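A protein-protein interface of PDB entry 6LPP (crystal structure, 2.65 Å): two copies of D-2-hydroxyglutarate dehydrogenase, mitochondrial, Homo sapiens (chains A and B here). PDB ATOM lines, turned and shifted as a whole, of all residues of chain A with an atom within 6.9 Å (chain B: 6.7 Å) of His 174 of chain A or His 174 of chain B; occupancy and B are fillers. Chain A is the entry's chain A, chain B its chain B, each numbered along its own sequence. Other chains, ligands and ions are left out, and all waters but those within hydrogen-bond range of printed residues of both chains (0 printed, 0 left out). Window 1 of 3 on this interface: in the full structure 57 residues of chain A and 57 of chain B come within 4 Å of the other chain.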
ATOM      1  N   VAL A 158      16.599 -12.286 -17.110  1.00  0.00           N
ATOM      2  CA  VAL A 158      15.210 -12.541 -17.480  1.00  0.00           C
ATOM      3  C   VAL A 158      14.433 -13.138 -16.308  1.00  0.00           C
ATOM      4  O   VAL A 158      13.293 -12.738 -16.036  1.00  0.00           O
ATOM      5  CB  VAL A 158      15.145 -13.448 -18.722  1.00  0.00           C
ATOM      6  CG1 VAL A 158      13.699 -13.728 -19.097  1.00  0.00           C
ATOM      7  CG2 VAL A 158      15.876 -12.801 -19.886  1.00  0.00           C
ATOM      8  N   ASN A 161      13.679 -10.383 -13.988  1.00  0.00           N
ATOM      9  CA  ASN A 161      13.161  -9.178 -14.637  1.00  0.00           C
ATOM     10  C   ASN A 161      13.996  -7.958 -14.240  1.00  0.00           C
ATOM     11  O   ASN A 161      13.506  -6.979 -13.673  1.00  0.00           O
ATOM     12  CB  ASN A 161      11.677  -8.972 -14.319  1.00  0.00           C
ATOM     13  CG  ASN A 161      11.080  -7.788 -15.057  1.00  0.00           C
ATOM     14  OD1 ASN A 161      11.427  -7.523 -16.208  1.00  0.00           O
ATOM     15  ND2 ASN A 161      10.182  -7.066 -14.396  1.00  0.00           N
ATOM     16  N   GLY A 171      13.125   0.375 -21.294  1.00  0.00           N
ATOM     17  CA  GLY A 171      12.016  -0.257 -20.611  1.00  0.00           C
ATOM     18  C   GLY A 171      12.262  -1.708 -20.232  1.00  0.00           C
ATOM     19  O   GLY A 171      13.393  -2.204 -20.182  1.00  0.00           O
ATOM     20  N   SER A 172      11.157  -2.397 -19.970  1.00  0.00           N
ATOM     21  CA  SER A 172      11.183  -3.677 -19.283  1.00  0.00           C
ATOM     22  C   SER A 172      11.582  -4.804 -20.226  1.00  0.00           C
ATOM     23  O   SER A 172      11.371  -4.737 -21.440  1.00  0.00           O
ATOM     24  CB  SER A 172       9.815  -3.978 -18.668  1.00  0.00           C
ATOM     25  OG  SER A 172       9.796  -5.260 -18.065  1.00  0.00           O
ATOM     26  N   LEU A 173      12.179  -5.848 -19.645  1.00  0.00           N
ATOM     27  CA  LEU A 173      12.368  -7.097 -20.373  1.00  0.00           C
ATOM     28  C   LEU A 173      11.036  -7.694 -20.811  1.00  0.00           C
ATOM     29  O   LEU A 173      10.983  -8.426 -21.806  1.00  0.00           O
ATOM     30  CB  LEU A 173      13.148  -8.092 -19.514  1.00  0.00           C
ATOM     31  CG  LEU A 173      14.610  -7.714 -19.272  1.00  0.00           C
ATOM     32  CD1 LEU A 173      15.224  -8.575 -18.178  1.00  0.00           C
ATOM     33  CD2 LEU A 173      15.412  -7.822 -20.561  1.00  0.00           C
ATOM     34  N   HIS A 174       9.956  -7.406 -20.079  1.00  0.00           N
ATOM     35  CA  HIS A 174       8.624  -7.796 -20.535  1.00  0.00           C
ATOM     36  C   HIS A 174       8.317  -7.240 -21.919  1.00  0.00           C
ATOM     37  O   HIS A 174       7.526  -7.832 -22.663  1.00  0.00           O
ATOM     38  CB  HIS A 174       7.561  -7.330 -19.537  1.00  0.00           C
ATOM     39  CG  HIS A 174       7.581  -8.071 -18.237  1.00  0.00           C
ATOM     40  ND1 HIS A 174       7.172  -9.383 -18.123  1.00  0.00           N
ATOM     41  CD2 HIS A 174       7.954  -7.684 -16.995  1.00  0.00           C
ATOM     42  CE1 HIS A 174       7.297  -9.773 -16.867  1.00  0.00           C
ATOM     43  NE2 HIS A 174       7.768  -8.761 -16.162  1.00  0.00           N
ATOM     44  N   GLY A 175       8.924  -6.113 -22.282  1.00  0.00           N
ATOM     45  CA  GLY A 175       8.802  -5.585 -23.626  1.00  0.00           C
ATOM     46  C   GLY A 175       9.910  -5.976 -24.582  1.00  0.00           C
ATOM     47  O   GLY A 175       9.654  -6.175 -25.774  1.00  0.00           O
ATOM     48  N   THR A 176      11.145  -6.090 -24.090  1.00  0.00           N
ATOM     49  CA  THR A 176      12.282  -6.300 -24.979  1.00  0.00           C
ATOM     50  C   THR A 176      12.592  -7.769 -25.238  1.00  0.00           C
ATOM     51  O   THR A 176      13.236  -8.077 -26.247  1.00  0.00           O
ATOM     52  CB  THR A 176      13.535  -5.625 -24.412  1.00  0.00           C
ATOM     53  OG1 THR A 176      13.824  -6.159 -23.115  1.00  0.00           O
ATOM     54  CG2 THR A 176      13.326  -4.123 -24.302  1.00  0.00           C
ATOM     55  N   VAL A 177      12.157  -8.677 -24.370  1.00  0.00           N
ATOM     56  CA  VAL A 177      12.340 -10.104 -24.613  1.00  0.00           C
ATOM     57  C   VAL A 177      11.310 -10.556 -25.639  1.00  0.00           C
ATOM     58  O   VAL A 177      10.104 -10.370 -25.446  1.00  0.00           O
ATOM     59  CB  VAL A 177      12.221 -10.914 -23.316  1.00  0.00           C
ATOM     60  CG1 VAL A 177      12.177 -12.402 -23.625  1.00  0.00           C
ATOM     61  CG2 VAL A 177      13.383 -10.597 -22.388  1.00  0.00           C
ATOM     62  N   LEU A 178      11.784 -11.135 -26.739  1.00  0.00           N
ATOM     63  CA  LEU A 178      10.895 -11.623 -27.785  1.00  0.00           C
ATOM     64  C   LEU A 178      10.569 -13.104 -27.662  1.00  0.00           C
ATOM     65  O   LEU A 178       9.491 -13.522 -28.095  1.00  0.00           O
ATOM     66  CB  LEU A 178      11.496 -11.347 -29.166  1.00  0.00           C
ATOM     67  CG  LEU A 178      11.815  -9.876 -29.445  1.00  0.00           C
ATOM     68  CD1 LEU A 178      12.538  -9.719 -30.770  1.00  0.00           C
ATOM     69  CD2 LEU A 178      10.542  -9.041 -29.427  1.00  0.00           C
ATOM     70  N   ASN A 200       0.711 -12.222 -31.908  1.00  0.00           N
ATOM     71  CA  ASN A 200      -0.468 -12.377 -31.052  1.00  0.00           C
ATOM     72  C   ASN A 200      -1.228 -13.660 -31.371  1.00  0.00           C
ATOM     73  O   ASN A 200      -2.441 -13.642 -31.583  1.00  0.00           O
ATOM     74  CB  ASN A 200      -1.378 -11.161 -31.180  1.00  0.00           C
ATOM     75  CG  ASN A 200      -0.887  -9.979 -30.374  1.00  0.00           C
ATOM     76  OD1 ASN A 200       0.075 -10.087 -29.615  1.00  0.00           O
ATOM     77  ND2 ASN A 200      -1.560  -8.843 -30.520  1.00  0.00           N
ATOM     78  N   TYR A 203      -1.753 -16.952 -25.887  1.00  0.00           N
ATOM     79  CA  TYR A 203      -1.269 -16.351 -24.653  1.00  0.00           C
ATOM     80  C   TYR A 203       0.239 -16.152 -24.720  1.00  0.00           C
ATOM     81  O   TYR A 203       0.969 -16.964 -25.296  1.00  0.00           O
ATOM     82  CB  TYR A 203      -1.607 -17.220 -23.438  1.00  0.00           C
ATOM     83  CG  TYR A 203      -3.062 -17.599 -23.264  1.00  0.00           C
ATOM     84  CD1 TYR A 203      -4.084 -16.803 -23.766  1.00  0.00           C
ATOM     85  CD2 TYR A 203      -3.413 -18.744 -22.559  1.00  0.00           C
ATOM     86  CE1 TYR A 203      -5.412 -17.152 -23.591  1.00  0.00           C
ATOM     87  CE2 TYR A 203      -4.733 -19.099 -22.377  1.00  0.00           C
ATOM     88  CZ  TYR A 203      -5.729 -18.301 -22.895  1.00  0.00           C
ATOM     89  OH  TYR A 203      -7.045 -18.655 -22.712  1.00  0.00           O
ATOM     90  N   ASP A 204       0.702 -15.053 -24.125  1.00  0.00           N
ATOM     91  CA  ASP A 204       2.122 -14.706 -24.102  1.00  0.00           C
ATOM     92  C   ASP A 204       2.782 -15.459 -22.945  1.00  0.00           C
ATOM     93  O   ASP A 204       3.149 -14.898 -21.912  1.00  0.00           O
ATOM     94  CB  ASP A 204       2.301 -13.198 -23.986  1.00  0.00           C
ATOM     95  CG  ASP A 204       3.684 -12.742 -24.402  1.00  0.00           C
ATOM     96  OD1 ASP A 204       4.535 -13.608 -24.692  1.00  0.00           O
ATOM     97  OD2 ASP A 204       3.917 -11.515 -24.445  1.00  0.00           O
ATOM     98  N   LYS A 206       5.616 -16.755 -22.379  1.00  0.00           N
ATOM     99  CA  LYS A 206       6.959 -16.403 -21.931  1.00  0.00           C
ATOM    100  C   LYS A 206       6.910 -15.411 -20.777  1.00  0.00           C
ATOM    101  O   LYS A 206       7.803 -15.407 -19.922  1.00  0.00           O
ATOM    102  CB  LYS A 206       7.773 -15.844 -23.101  1.00  0.00           C
ATOM    103  CG  LYS A 206       7.381 -14.437 -23.520  1.00  0.00           C
ATOM    104  CD  LYS A 206       8.181 -13.956 -24.714  1.00  0.00           C
ATOM    105  CE  LYS A 206       7.827 -12.517 -25.047  1.00  0.00           C
ATOM    106  NZ  LYS A 206       6.577 -12.425 -25.851  1.00  0.00           N
ATOM    107  N   GLN A 207       5.891 -14.548 -20.757  1.00  0.00           N
ATOM    108  CA  GLN A 207       5.761 -13.548 -19.706  1.00  0.00           C
ATOM    109  C   GLN A 207       5.733 -14.179 -18.318  1.00  0.00           C
ATOM    110  O   GLN A 207       6.231 -13.579 -17.359  1.00  0.00           O
ATOM    111  CB  GLN A 207       4.495 -12.719 -19.930  1.00  0.00           C
ATOM    112  CG  GLN A 207       4.492 -11.884 -21.202  1.00  0.00           C
ATOM    113  CD  GLN A 207       5.477 -10.732 -21.170  1.00  0.00           C
ATOM    114  OE1 GLN A 207       6.107 -10.458 -20.148  1.00  0.00           O
ATOM    115  NE2 GLN A 207       5.608 -10.042 -22.297  1.00  0.00           N
ATOM    116  N   LEU A 208       5.152 -15.379 -18.188  1.00  0.00           N
ATOM    117  CA  LEU A 208       5.156 -16.060 -16.895  1.00  0.00           C
ATOM    118  C   LEU A 208       6.561 -16.306 -16.368  1.00  0.00           C
ATOM    119  O   LEU A 208       6.771 -16.314 -15.150  1.00  0.00           O
ATOM    120  CB  LEU A 208       4.406 -17.389 -16.989  1.00  0.00           C
ATOM    121  CG  LEU A 208       2.892 -17.300 -17.109  1.00  0.00           C
ATOM    122  CD1 LEU A 208       2.294 -18.687 -17.236  1.00  0.00           C
ATOM    123  CD2 LEU A 208       2.368 -16.605 -15.869  1.00  0.00           C
ATOM    124  N   PHE A 209       7.531 -16.505 -17.251  1.00  0.00           N
ATOM    125  CA  PHE A 209       8.869 -16.860 -16.808  1.00  0.00           C
ATOM    126  C   PHE A 209       9.772 -15.650 -16.623  1.00  0.00           C
ATOM    127  O   PHE A 209      10.880 -15.799 -16.096  1.00  0.00           O
ATOM    128  CB  PHE A 209       9.485 -17.865 -17.783  1.00  0.00           C
ATOM    129  CG  PHE A 209       8.675 -19.120 -17.922  1.00  0.00           C
ATOM    130  CD1 PHE A 209       8.827 -20.158 -17.017  1.00  0.00           C
ATOM    131  CD2 PHE A 209       7.729 -19.245 -18.924  1.00  0.00           C
ATOM    132  CE1 PHE A 209       8.072 -21.309 -17.126  1.00  0.00           C
ATOM    133  CE2 PHE A 209       6.968 -20.393 -19.036  1.00  0.00           C
ATOM    134  CZ  PHE A 209       7.141 -21.427 -18.136  1.00  0.00           C
ATOM    135  N   ILE A 210       9.326 -14.467 -17.032  1.00  0.00           N
ATOM    136  CA  ILE A 210      10.090 -13.243 -16.831  1.00  0.00           C
ATOM    137  C   ILE A 210       9.714 -12.707 -15.454  1.00  0.00           C
ATOM    138  O   ILE A 210       8.577 -12.283 -15.232  1.00  0.00           O
ATOM    139  CB  ILE A 210       9.800 -12.211 -17.926  1.00  0.00           C
ATOM    140  CG1 ILE A 210      10.096 -12.797 -19.309  1.00  0.00           C
ATOM    141  CG2 ILE A 210      10.606 -10.943 -17.690  1.00  0.00           C
ATOM    142  CD1 ILE A 210       9.624 -11.926 -20.455  1.00  0.00           C
ATOM    143  N   GLY A 211      10.668 -12.727 -14.529  1.00  0.00           N
ATOM    144  CA  GLY A 211      10.395 -12.402 -13.146  1.00  0.00           C
ATOM    145  C   GLY A 211       9.965 -13.560 -12.271  1.00  0.00           C
ATOM    146  O   GLY A 211       9.611 -13.332 -11.109  1.00  0.00           O
ATOM    147  N   VAL B 158      -6.072  -3.797 -24.391  1.00  0.00           N
ATOM    148  CA  VAL B 158      -5.273  -4.655 -23.519  1.00  0.00           C
ATOM    149  C   VAL B 158      -5.594  -6.127 -23.759  1.00  0.00           C
ATOM    150  O   VAL B 158      -4.689  -6.967 -23.842  1.00  0.00           O
ATOM    151  CB  VAL B 158      -5.476  -4.261 -22.045  1.00  0.00           C
ATOM    152  CG1 VAL B 158      -4.720  -5.216 -21.126  1.00  0.00           C
ATOM    153  CG2 VAL B 158      -5.025  -2.827 -21.810  1.00  0.00           C
ATOM    154  N   ASN B 161      -4.021  -7.195 -26.890  1.00  0.00           N
ATOM    155  CA  ASN B 161      -2.631  -6.749 -27.014  1.00  0.00           C
ATOM    156  C   ASN B 161      -2.425  -5.979 -28.323  1.00  0.00           C
ATOM    157  O   ASN B 161      -1.568  -6.307 -29.148  1.00  0.00           O
ATOM    158  CB  ASN B 161      -1.669  -7.935 -26.896  1.00  0.00           C
ATOM    159  CG  ASN B 161      -0.216  -7.520 -26.943  1.00  0.00           C
ATOM    160  OD1 ASN B 161       0.156  -6.463 -26.436  1.00  0.00           O
ATOM    161  ND2 ASN B 161       0.620  -8.358 -27.548  1.00  0.00           N
ATOM    162  N   GLY B 171       6.392   0.751 -28.149  1.00  0.00           N
ATOM    163  CA  GLY B 171       6.400  -0.667 -27.846  1.00  0.00           C
ATOM    164  C   GLY B 171       5.073  -1.256 -27.393  1.00  0.00           C
ATOM    165  O   GLY B 171       4.001  -0.649 -27.478  1.00  0.00           O
ATOM    166  N   SER B 172       5.174  -2.489 -26.900  1.00  0.00           N
ATOM    167  CA  SER B 172       4.010  -3.297 -26.563  1.00  0.00           C
ATOM    168  C   SER B 172       3.302  -2.810 -25.303  1.00  0.00           C
ATOM    169  O   SER B 172       3.900  -2.190 -24.419  1.00  0.00           O
ATOM    170  CB  SER B 172       4.419  -4.759 -26.383  1.00  0.00           C
ATOM    171  OG  SER B 172       3.324  -5.548 -25.953  1.00  0.00           O
ATOM    172  N   LEU B 173       2.000  -3.107 -25.237  1.00  0.00           N
ATOM    173  CA  LEU B 173       1.243  -2.964 -23.996  1.00  0.00           C
ATOM    174  C   LEU B 173       1.807  -3.838 -22.881  1.00  0.00           C
ATOM    175  O   LEU B 173       1.655  -3.508 -21.700  1.00  0.00           O
ATOM    176  CB  LEU B 173      -0.229  -3.299 -24.236  1.00  0.00           C
ATOM    177  CG  LEU B 173      -1.025  -2.307 -25.085  1.00  0.00           C
ATOM    178  CD1 LEU B 173      -2.403  -2.864 -25.409  1.00  0.00           C
ATOM    179  CD2 LEU B 173      -1.137  -0.968 -24.371  1.00  0.00           C
ATOM    180  N   HIS B 174       2.445  -4.958 -23.233  1.00  0.00           N
ATOM    181  CA  HIS B 174       3.149  -5.756 -22.233  1.00  0.00           C
ATOM    182  C   HIS B 174       4.203  -4.940 -21.495  1.00  0.00           C
ATOM    183  O   HIS B 174       4.546  -5.261 -20.352  1.00  0.00           O
ATOM    184  CB  HIS B 174       3.801  -6.974 -22.892  1.00  0.00           C
ATOM    185  CG  HIS B 174       2.828  -8.008 -23.368  1.00  0.00           C
ATOM    186  ND1 HIS B 174       2.168  -8.861 -22.508  1.00  0.00           N
ATOM    187  CD2 HIS B 174       2.410  -8.334 -24.614  1.00  0.00           C
ATOM    188  CE1 HIS B 174       1.385  -9.666 -23.204  1.00  0.00           C
ATOM    189  NE2 HIS B 174       1.511  -9.365 -24.485  1.00  0.00           N
ATOM    190  N   GLY B 175       4.725  -3.892 -22.125  1.00  0.00           N
ATOM    191  CA  GLY B 175       5.613  -2.961 -21.453  1.00  0.00           C
ATOM    192  C   GLY B 175       4.951  -1.738 -20.851  1.00  0.00           C
ATOM    193  O   GLY B 175       5.357  -1.279 -19.780  1.00  0.00           O
ATOM    194  N   THR B 176       3.927  -1.202 -21.516  1.00  0.00           N
ATOM    195  CA  THR B 176       3.353   0.074 -21.105  1.00  0.00           C
ATOM    196  C   THR B 176       2.202  -0.063 -20.118  1.00  0.00           C
ATOM    197  O   THR B 176       1.901   0.903 -19.409  1.00  0.00           O
ATOM    198  CB  THR B 176       2.861   0.861 -22.325  1.00  0.00           C
ATOM    199  OG1 THR B 176       1.980   0.044 -23.102  1.00  0.00           O
ATOM    200  CG2 THR B 176       4.039   1.289 -23.189  1.00  0.00           C
ATOM    201  N   VAL B 177       1.553  -1.224 -20.048  1.00  0.00           N
ATOM    202  CA  VAL B 177       0.543  -1.434 -19.018  1.00  0.00           C
ATOM    203  C   VAL B 177       1.252  -1.631 -17.687  1.00  0.00           C
ATOM    204  O   VAL B 177       2.078  -2.538 -17.533  1.00  0.00           O
ATOM    205  CB  VAL B 177      -0.354  -2.634 -19.352  1.00  0.00           C
ATOM    206  CG1 VAL B 177      -1.278  -2.939 -18.183  1.00  0.00           C
ATOM    207  CG2 VAL B 177      -1.163  -2.365 -20.612  1.00  0.00           C
ATOM    208  N   ASN B 200       8.800  -5.724  -8.655  1.00  0.00           N
ATOM    209  CA  ASN B 200       9.118  -7.145  -8.792  1.00  0.00           C
ATOM    210  C   ASN B 200       8.771  -7.907  -7.513  1.00  0.00           C
ATOM    211  O   ASN B 200       9.604  -8.591  -6.917  1.00  0.00           O
ATOM    212  CB  ASN B 200      10.587  -7.325  -9.162  1.00  0.00           C
ATOM    213  CG  ASN B 200      10.852  -7.087 -10.634  1.00  0.00           C
ATOM    214  OD1 ASN B 200       9.924  -6.973 -11.434  1.00  0.00           O
ATOM    215  ND2 ASN B 200      12.126  -7.025 -11.003  1.00  0.00           N
ATOM    216  N   ASP B 204       4.310 -11.577 -12.459  1.00  0.00           N
ATOM    217  CA  ASP B 204       3.667 -10.476 -13.174  1.00  0.00           C
ATOM    218  C   ASP B 204       2.345 -10.994 -13.745  1.00  0.00           C
ATOM    219  O   ASP B 204       2.187 -11.236 -14.945  1.00  0.00           O
ATOM    220  CB  ASP B 204       4.586  -9.930 -14.258  1.00  0.00           C
ATOM    221  CG  ASP B 204       4.221  -8.521 -14.675  1.00  0.00           C
ATOM    222  OD1 ASP B 204       3.263  -7.959 -14.104  1.00  0.00           O
ATOM    223  OD2 ASP B 204       4.896  -7.972 -15.572  1.00  0.00           O
ATOM    224  N   LYS B 206      -0.552  -9.767 -14.305  1.00  0.00           N
ATOM    225  CA  LYS B 206      -1.285  -8.992 -15.300  1.00  0.00           C
ATOM    226  C   LYS B 206      -0.915  -9.400 -16.719  1.00  0.00           C
ATOM    227  O   LYS B 206      -1.754  -9.318 -17.626  1.00  0.00           O
ATOM    228  CB  LYS B 206      -1.030  -7.501 -15.077  1.00  0.00           C
ATOM    229  CG  LYS B 206       0.369  -7.048 -15.463  1.00  0.00           C
ATOM    230  CD  LYS B 206       0.547  -5.552 -15.298  1.00  0.00           C
ATOM    231  CE  LYS B 206       1.949  -5.130 -15.701  1.00  0.00           C
ATOM    232  NZ  LYS B 206       2.933  -5.353 -14.605  1.00  0.00           N
ATOM    233  N   GLN B 207       0.322  -9.860 -16.926  1.00  0.00           N
ATOM    234  CA  GLN B 207       0.752 -10.246 -18.263  1.00  0.00           C
ATOM    235  C   GLN B 207      -0.124 -11.350 -18.840  1.00  0.00           C
ATOM    236  O   GLN B 207      -0.342 -11.391 -20.056  1.00  0.00           O
ATOM    237  CB  GLN B 207       2.215 -10.693 -18.231  1.00  0.00           C
ATOM    238  CG  GLN B 207       3.220  -9.608 -17.856  1.00  0.00           C
ATOM    239  CD  GLN B 207       3.233  -8.438 -18.825  1.00  0.00           C
ATOM    240  OE1 GLN B 207       2.784  -8.553 -19.965  1.00  0.00           O
ATOM    241  NE2 GLN B 207       3.754  -7.304 -18.373  1.00  0.00           N
ATOM    242  N   LEU B 208      -0.633 -12.252 -17.991  1.00  0.00           N
ATOM    243  CA  LEU B 208      -1.513 -13.307 -18.491  1.00  0.00           C
ATOM    244  C   LEU B 208      -2.755 -12.749 -19.167  1.00  0.00           C
ATOM    245  O   LEU B 208      -3.279 -13.362 -20.103  1.00  0.00           O
ATOM    246  CB  LEU B 208      -1.914 -14.250 -17.359  1.00  0.00           C
ATOM    247  CG  LEU B 208      -0.808 -15.150 -16.822  1.00  0.00           C
ATOM    248  CD1 LEU B 208      -1.123 -15.597 -15.405  1.00  0.00           C
ATOM    249  CD2 LEU B 208      -0.644 -16.346 -17.747  1.00  0.00           C
ATOM    250  N   PHE B 209      -3.236 -11.592 -18.720  1.00  0.00           N
ATOM    251  CA  PHE B 209      -4.470 -11.031 -19.249  1.00  0.00           C
ATOM    252  C   PHE B 209      -4.247 -10.096 -20.428  1.00  0.00           C
ATOM    253  O   PHE B 209      -5.220  -9.704 -21.081  1.00  0.00           O
ATOM    254  CB  PHE B 209      -5.232 -10.322 -18.127  1.00  0.00           C
ATOM    255  CG  PHE B 209      -5.510 -11.213 -16.952  1.00  0.00           C
ATOM    256  CD1 PHE B 209      -6.578 -12.091 -16.971  1.00  0.00           C
ATOM    257  CD2 PHE B 209      -4.677 -11.202 -15.846  1.00  0.00           C
ATOM    258  CE1 PHE B 209      -6.828 -12.927 -15.900  1.00  0.00           C
ATOM    259  CE2 PHE B 209      -4.921 -12.035 -14.773  1.00  0.00           C
ATOM    260  CZ  PHE B 209      -5.998 -12.898 -14.799  1.00  0.00           C
ATOM    261  N   ILE B 210      -3.001  -9.734 -20.715  1.00  0.00           N
ATOM    262  CA  ILE B 210      -2.681  -8.929 -21.889  1.00  0.00           C
ATOM    263  C   ILE B 210      -2.577  -9.875 -23.081  1.00  0.00           C
ATOM    264  O   ILE B 210      -1.680 -10.720 -23.140  1.00  0.00           O
ATOM    265  CB  ILE B 210      -1.387  -8.133 -21.691  1.00  0.00           C
ATOM    266  CG1 ILE B 210      -1.506  -7.236 -20.458  1.00  0.00           C
ATOM    267  CG2 ILE B 210      -1.086  -7.296 -22.925  1.00  0.00           C
ATOM    268  CD1 ILE B 210      -0.257  -6.447 -20.158  1.00  0.00           C
ATOM    269  N   GLY B 211      -3.492  -9.731 -24.036  1.00  0.00           N
ATOM    270  CA  GLY B 211      -3.542 -10.607 -25.189  1.00  0.00           C
ATOM    271  C   GLY B 211      -4.339 -11.883 -25.014  1.00  0.00           C
ATOM    272  O   GLY B 211      -4.335 -12.721 -25.923  1.00  0.00           O
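Hydrophobic or aromatic side chains of chain B that line the printed part of chain A: His 174 and Leu 208. Hydrophobic or aromatic side chains of chain A within 4 Å of the printed part of chain B: His 174 and Leu 208. Among the printed residues, no Asp or Glu carboxylate lies within 4 Å of a Lys or Arg side-chain nitrogen of the other chain.
ND2 of Asn 161 of chain A sits at hydrogen-bond distance from OD1 of Asn 200 of chain B, 3.0 Å away. The side-chain amide nitrogen of Asn 161 of chain B sits at hydrogen-bond distance from the side-chain amide oxygen of Asn 200 of chain A, at 2.7 Å. OD2 of Asp 204 of chain A sits at hydrogen-bond distance from NE2 of His 174 of chain B, 3.2 Å away. A ring nitrogen (NE2) of His 174 of chain A lies within hydrogen-bond range of the side-chain carboxylate (OD2) of Asp 204 of chain B (3.0 Å).
NE2 of Gln 207 of chain B lies within hydrogen-bond range of OD2 of Asp 204 of chain B, 3.1 Å away. NE2 of Gln 207 of chain A lies within hydrogen-bond range of OD2 of Asp 204 of chain A. OG of Ser 172 of chain A is in hydrogen-bond range of N of His 174 of chain A. The side-chain carboxylate of Asp 204 of chain B is in salt-bridge range of the side-chain amino group of Lys 206 of chain B (2.7 Å). The side-chain amide oxygen (OE1) of Gln 207 of chain B sits at hydrogen-bond distance from a ring nitrogen (ND1) of His 174 of chain B, 2.6 Å away. OD1 of Asn 161 of chain A lies within hydrogen-bond range of OG of Ser 172 of chain A.
His 174 of chain B touches its own counterpart, His 174 of chain A. His 174 of chain A touches Asp 204 of chain B, and with the chains exchanged Asp 204 of chain A touches His 174 of chain B. Gln 207 of chain B touches its own counterpart, Gln 207 of chain A. Leu 208 of chain B touches its own counterpart, Leu 208 of chain A. Positions printed for both chains: 158, 161, 171, 172, 173, 174, 175, 176, 177, 200, 204, 206, 207, 208, 209, 210 and 211.
Among the printed residues, pairs that only touch across the chains: Gln 207 of chain A with Gln 207 of chain B, Leu 208 of chain A with Leu 208 of chain B, Gln 207 of chain A with His 174 of chain B, His 174 of chain A with His 174 of chain B and His 174 of chain A with Gln 207 of chain B.
Printed residues of chain B within 4 Å of His 174 of chain A: His 174 (3.7 Å), Asp 204 (3.0 Å) and Gln 207 (3.9 Å). Printed residues of chain B within 4 Å of Asp 204 of chain A: His 174. Of the printed residues of chain B, Leu 208 of chain A touches Leu 208. Val 158 of chain B touches none of the printed residues of chain A. Of chain A, only His 174 (3.7 Å), Asp 204 (3.2 Å) and Gln 207 (3.6 Å) come within 4 Å of His 174 of chain B. Of the printed residues of chain A, Asn 200 of chain B touches Asn 161 (3.0 Å). Of the printed residues of chain A, Leu 208 of chain B touches Leu 208. The nearest residue of chain B that does not touch His 174 of chain A is Gly 175 of chain B (4.9 Å). The nearest residue of chain A that does not touch His 174 of chain B is Gly 175 of chain A (4.9 Å). The nearest printed residue of chain B that does not touch Asp 204 of chain A is Ile 210 of chain B (4.8 Å).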
